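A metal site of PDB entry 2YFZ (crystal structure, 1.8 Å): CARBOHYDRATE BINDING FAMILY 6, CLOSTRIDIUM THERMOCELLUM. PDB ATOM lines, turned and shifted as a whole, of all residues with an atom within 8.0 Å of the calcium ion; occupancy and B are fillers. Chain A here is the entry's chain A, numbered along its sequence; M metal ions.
The side-chain amide oxygen (OD1) of Asn 34 lies close to the side-chain carboxylate (OD1) of Asp 32 (2.9 Å).
N of Ala 132 is in hydrogen-bond range of O of Cys 65, 2.7 Å away.
The backbone NH (N) of Cys 65 sits at hydrogen-bond distance from the backbone carbonyl oxygen (O) of Glu 133, at 3.0 Å.
The backbone NH of Gly 31 sits at hydrogen-bond distance from the side-chain carboxylate of Glu 133 (2.6 Å).
The nearest printed residue that does not touch the calcium ion is Ala 28 (4.3 Å).
The calcium ion is bound by the backbone carbonyl oxygen of Lys 27 (2.3 Å), the backbone carbonyl oxygen of Asp 32 (2.4 Å), the backbone carbonyl oxygen of Ala 132 (2.4 Å), the side-chain hydroxyl of Thr 35 (2.5 Å), the side-chain carboxylate of Asp 30 (2.5 Å), the side-chain carboxylate of Glu 133 (2.5 Å) and the backbone carbonyl oxygen of Thr 35 (2.7 Å).
The calcium ion has seven donor atoms within binding distance.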
ATOM      1  N   THR A  24      21.940  12.693   6.062  1.00  0.00           N
ATOM      2  CA  THR A  24      21.833  11.738   7.185  1.00  0.00           C
ATOM      3  C   THR A  24      22.243  10.324   6.723  1.00  0.00           C
ATOM      4  O   THR A  24      22.540  10.109   5.528  1.00  0.00           O
ATOM      5  CB  THR A  24      20.404  11.635   7.685  1.00  0.00           C
ATOM      6  OG1 THR A  24      19.612  11.043   6.640  1.00  0.00           O
ATOM      7  CG2 THR A  24      19.816  13.056   8.071  1.00  0.00           C
ATOM      8  N   ILE A  25      22.224   9.363   7.648  1.00  0.00           N
ATOM      9  CA  ILE A  25      22.566   7.966   7.330  1.00  0.00           C
ATOM     10  C   ILE A  25      21.711   7.389   6.210  1.00  0.00           C
ATOM     11  O   ILE A  25      22.131   6.453   5.526  1.00  0.00           O
ATOM     12  CB  ILE A  25      22.498   7.067   8.577  1.00  0.00           C
ATOM     13  CG1 ILE A  25      21.110   7.166   9.237  1.00  0.00           C
ATOM     14  CG2 ILE A  25      23.600   7.500   9.548  1.00  0.00           C
ATOM     15  CD1 ILE A  25      20.962   6.343  10.575  1.00  0.00           C
ATOM     16  N   HIS A  26      20.498   7.925   6.025  1.00  0.00           N
ATOM     17  CA  HIS A  26      19.633   7.436   4.958  1.00  0.00           C
ATOM     18  C   HIS A  26      20.199   7.610   3.559  1.00  0.00           C
ATOM     19  O   HIS A  26      19.822   6.848   2.655  1.00  0.00           O
ATOM     20  CB  HIS A  26      18.235   8.068   5.073  1.00  0.00           C
ATOM     21  CG  HIS A  26      17.471   7.543   6.246  1.00  0.00           C
ATOM     22  ND1 HIS A  26      16.651   6.437   6.172  1.00  0.00           N
ATOM     23  CD2 HIS A  26      17.473   7.936   7.553  1.00  0.00           C
ATOM     24  CE1 HIS A  26      16.149   6.190   7.371  1.00  0.00           C
ATOM     25  NE2 HIS A  26      16.640   7.078   8.225  1.00  0.00           N
ATOM     26  N   LYS A  27      21.125   8.559   3.385  1.00  0.00           N
ATOM     27  CA  LYS A  27      21.763   8.758   2.088  1.00  0.00           C
ATOM     28  C   LYS A  27      22.612   7.579   1.660  1.00  0.00           C
ATOM     29  O   LYS A  27      22.924   7.442   0.458  1.00  0.00           O
ATOM     30  CB  LYS A  27      22.648  10.007   2.074  1.00  0.00           C
ATOM     31  CG  LYS A  27      21.946  11.342   2.396  1.00  0.00           C
ATOM     32  CD  LYS A  27      20.756  11.576   1.469  1.00  0.00           C
ATOM     33  CE  LYS A  27      20.211  12.954   1.714  1.00  0.00           C
ATOM     34  NZ  LYS A  27      18.856  13.077   1.102  1.00  0.00           N
ATOM     35  N   ALA A  28      22.999   6.705   2.595  1.00  0.00           N
ATOM     36  CA  ALA A  28      23.827   5.548   2.248  1.00  0.00           C
ATOM     37  C   ALA A  28      23.012   4.350   1.769  1.00  0.00           C
ATOM     38  O   ALA A  28      23.585   3.303   1.413  1.00  0.00           O
ATOM     39  CB  ALA A  28      24.713   5.134   3.457  1.00  0.00           C
ATOM     40  N   PHE A  29      21.681   4.503   1.735  1.00  0.00           N
ATOM     41  CA  PHE A  29      20.812   3.407   1.353  1.00  0.00           C
ATOM     42  C   PHE A  29      19.870   3.776   0.213  1.00  0.00           C
ATOM     43  O   PHE A  29      18.869   3.090  -0.011  1.00  0.00           O
ATOM     44  CB  PHE A  29      20.014   2.903   2.567  1.00  0.00           C
ATOM     45  CG  PHE A  29      20.893   2.432   3.690  1.00  0.00           C
ATOM     46  CD1 PHE A  29      21.439   1.136   3.670  1.00  0.00           C
ATOM     47  CD2 PHE A  29      21.218   3.290   4.751  1.00  0.00           C
ATOM     48  CE1 PHE A  29      22.269   0.698   4.724  1.00  0.00           C
ATOM     49  CE2 PHE A  29      22.057   2.841   5.806  1.00  0.00           C
ATOM     50  CZ  PHE A  29      22.572   1.550   5.777  1.00  0.00           C
ATOM     51  N   ASP A  30      20.172   4.855  -0.504  1.00  0.00           N
ATOM     52  CA  ASP A  30      19.193   5.383  -1.462  1.00  0.00           C
ATOM     53  C   ASP A  30      19.464   4.974  -2.911  1.00  0.00           C
ATOM     54  O   ASP A  30      18.713   5.401  -3.810  1.00  0.00           O
ATOM     55  CB  ASP A  30      19.066   6.910  -1.375  1.00  0.00           C
ATOM     56  CG  ASP A  30      20.347   7.642  -1.701  1.00  0.00           C
ATOM     57  OD1 ASP A  30      21.371   7.001  -2.036  1.00  0.00           O
ATOM     58  OD2 ASP A  30      20.328   8.884  -1.599  1.00  0.00           O
ATOM     59  N   GLY A  31      20.519   4.195  -3.127  1.00  0.00           N
ATOM     60  CA  GLY A  31      20.874   3.708  -4.476  1.00  0.00           C
ATOM     61  C   GLY A  31      21.585   4.734  -5.342  1.00  0.00           C
ATOM     62  O   GLY A  31      21.842   4.468  -6.510  1.00  0.00           O
ATOM     63  N   ASP A  32      21.907   5.901  -4.799  1.00  0.00           N
ATOM     64  CA  ASP A  32      22.577   6.953  -5.585  1.00  0.00           C
ATOM     65  C   ASP A  32      24.027   7.087  -5.091  1.00  0.00           C
ATOM     66  O   ASP A  32      24.260   7.400  -3.928  1.00  0.00           O
ATOM     67  CB  ASP A  32      21.843   8.278  -5.420  1.00  0.00           C
ATOM     68  CG  ASP A  32      22.383   9.383  -6.340  1.00  0.00           C
ATOM     69  OD1 ASP A  32      23.391   9.182  -7.021  1.00  0.00           O
ATOM     70  OD2 ASP A  32      21.747  10.455  -6.384  1.00  0.00           O
ATOM     71  N   LEU A  33      25.007   6.803  -5.945  1.00  0.00           N
ATOM     72  CA  LEU A  33      26.412   6.888  -5.514  1.00  0.00           C
ATOM     73  C   LEU A  33      26.877   8.337  -5.368  1.00  0.00           C
ATOM     74  O   LEU A  33      27.982   8.580  -4.865  1.00  0.00           O
ATOM     75  CB  LEU A  33      27.329   6.124  -6.484  1.00  0.00           C
ATOM     76  CG  LEU A  33      26.923   4.660  -6.775  1.00  0.00           C
ATOM     77  CD1 LEU A  33      28.038   4.040  -7.652  1.00  0.00           C
ATOM     78  CD2 LEU A  33      26.730   3.866  -5.436  1.00  0.00           C
ATOM     79  N   ASN A  34      26.037   9.286  -5.809  1.00  0.00           N
ATOM     80  CA  ASN A  34      26.332  10.706  -5.667  1.00  0.00           C
ATOM     81  C   ASN A  34      25.920  11.307  -4.312  1.00  0.00           C
ATOM     82  O   ASN A  34      26.368  12.401  -3.955  1.00  0.00           O
ATOM     83  CB  ASN A  34      25.636  11.522  -6.773  1.00  0.00           C
ATOM     84  CG  ASN A  34      26.048  11.074  -8.139  1.00  0.00           C
ATOM     85  OD1 ASN A  34      25.265  10.419  -8.857  1.00  0.00           O
ATOM     86  ND2 ASN A  34      27.289  11.369  -8.508  1.00  0.00           N
ATOM     87  N   THR A  35      25.055  10.635  -3.592  1.00  0.00           N
ATOM     88  CA  THR A  35      24.601  11.147  -2.287  1.00  0.00           C
ATOM     89  C   THR A  35      25.339  10.393  -1.200  1.00  0.00           C
ATOM     90  O   THR A  35      25.674   9.216  -1.374  1.00  0.00           O
ATOM     91  CB  THR A  35      23.110  10.927  -2.066  1.00  0.00           C
ATOM     92  OG1 THR A  35      22.823   9.531  -2.150  1.00  0.00           O
ATOM     93  CG2 THR A  35      22.257  11.700  -3.085  1.00  0.00           C
ATOM     94  N   PHE A  36      25.577  11.041  -0.054  1.00  0.00           N
ATOM     95  CA  PHE A  36      26.445  10.449   0.959  1.00  0.00           C
ATOM     96  C   PHE A  36      25.972  10.841   2.355  1.00  0.00           C
ATOM     97  O   PHE A  36      25.310  11.866   2.518  1.00  0.00           O
ATOM     98  CB  PHE A  36      27.910  10.934   0.778  1.00  0.00           C
ATOM     99  CG  PHE A  36      28.027  12.423   0.638  1.00  0.00           C
ATOM    100  CD1 PHE A  36      28.124  13.250   1.760  1.00  0.00           C
ATOM    101  CD2 PHE A  36      27.987  13.002  -0.634  1.00  0.00           C
ATOM    102  CE1 PHE A  36      28.175  14.668   1.611  1.00  0.00           C
ATOM    103  CE2 PHE A  36      28.052  14.396  -0.803  1.00  0.00           C
ATOM    104  CZ  PHE A  36      28.141  15.226   0.330  1.00  0.00           C
ATOM    105  N   PHE A  37      26.343  10.024   3.327  1.00  0.00           N
ATOM    106  CA  PHE A  37      26.177  10.359   4.753  1.00  0.00           C
ATOM    107  C   PHE A  37      27.328  11.269   5.158  1.00  0.00           C
ATOM    108  O   PHE A  37      28.502  10.935   4.917  1.00  0.00           O
ATOM    109  CB  PHE A  37      26.213   9.049   5.562  1.00  0.00           C
ATOM    110  CG  PHE A  37      26.281   9.244   7.070  1.00  0.00           C
ATOM    111  CD1 PHE A  37      25.494  10.197   7.722  1.00  0.00           C
ATOM    112  CD2 PHE A  37      27.149   8.432   7.829  1.00  0.00           C
ATOM    113  CE1 PHE A  37      25.574  10.389   9.120  1.00  0.00           C
ATOM    114  CE2 PHE A  37      27.244   8.592   9.238  1.00  0.00           C
ATOM    115  CZ  PHE A  37      26.442   9.578   9.879  1.00  0.00           C
ATOM    116  N   CYS A  65      30.444   2.195  -1.400  1.00  0.00           N
ATOM    117  CA  CYS A  65      31.004   3.231  -2.255  1.00  0.00           C
ATOM    118  C   CYS A  65      31.374   4.414  -1.345  1.00  0.00           C
ATOM    119  O   CYS A  65      30.572   4.826  -0.506  1.00  0.00           O
ATOM    120  CB  CYS A  65      29.950   3.672  -3.301  1.00  0.00           C
ATOM    121  SG  CYS A  65      30.558   5.015  -4.376  1.00  0.00           S
ATOM    122  N   ILE A 131      30.410   8.026   3.666  1.00  0.00           N
ATOM    123  CA  ILE A 131      30.192   6.862   2.833  1.00  0.00           C
ATOM    124  C   ILE A 131      29.026   7.215   1.914  1.00  0.00           C
ATOM    125  O   ILE A 131      28.074   7.873   2.362  1.00  0.00           O
ATOM    126  CB  ILE A 131      29.891   5.592   3.696  1.00  0.00           C
ATOM    127  CG1 ILE A 131      29.724   4.333   2.835  1.00  0.00           C
ATOM    128  CG2 ILE A 131      28.644   5.801   4.607  1.00  0.00           C
ATOM    129  CD1 ILE A 131      29.590   2.987   3.670  1.00  0.00           C
ATOM    130  N   ALA A 132      29.087   6.814   0.653  1.00  0.00           N
ATOM    131  CA  ALA A 132      27.975   7.134  -0.278  1.00  0.00           C
ATOM    132  C   ALA A 132      26.905   6.056  -0.353  1.00  0.00           C
ATOM    133  O   ALA A 132      25.719   6.371  -0.542  1.00  0.00           O
ATOM    134  CB  ALA A 132      28.516   7.452  -1.717  1.00  0.00           C
ATOM    135  N   GLU A 133      27.289   4.792  -0.272  1.00  0.00           N
ATOM    136  CA  GLU A 133      26.307   3.719  -0.426  1.00  0.00           C
ATOM    137  C   GLU A 133      26.822   2.483   0.306  1.00  0.00           C
ATOM    138  O   GLU A 133      28.032   2.195   0.300  1.00  0.00           O
ATOM    139  CB  GLU A 133      26.033   3.403  -1.908  1.00  0.00           C
ATOM    140  CG  GLU A 133      24.719   2.695  -2.144  1.00  0.00           C
ATOM    141  CD  GLU A 133      23.486   3.602  -1.915  1.00  0.00           C
ATOM    142  OE1 GLU A 133      23.591   4.855  -1.975  1.00  0.00           O
ATOM    143  OE2 GLU A 133      22.418   3.052  -1.711  1.00  0.00           O
ATOM    144  N   LEU A 134      25.901   1.761   0.934  1.00  0.00           N
ATOM    145  CA  LEU A 134      26.231   0.633   1.774  1.00  0.00           C
ATOM    146  C   LEU A 134      25.208  -0.452   1.514  1.00  0.00           C
ATOM    147  O   LEU A 134      24.001  -0.178   1.601  1.00  0.00           O
ATOM    148  CB  LEU A 134      26.167   1.045   3.256  1.00  0.00           C
ATOM    149  CG  LEU A 134      26.399  -0.111   4.256  1.00  0.00           C
ATOM    150  CD1 LEU A 134      27.752  -0.776   4.017  1.00  0.00           C
ATOM    151  CD2 LEU A 134      26.309   0.436   5.699  1.00  0.00           C
HETATM  152 CA    CA M   1      23.815   7.323  -1.620  1.00  0.00          CA
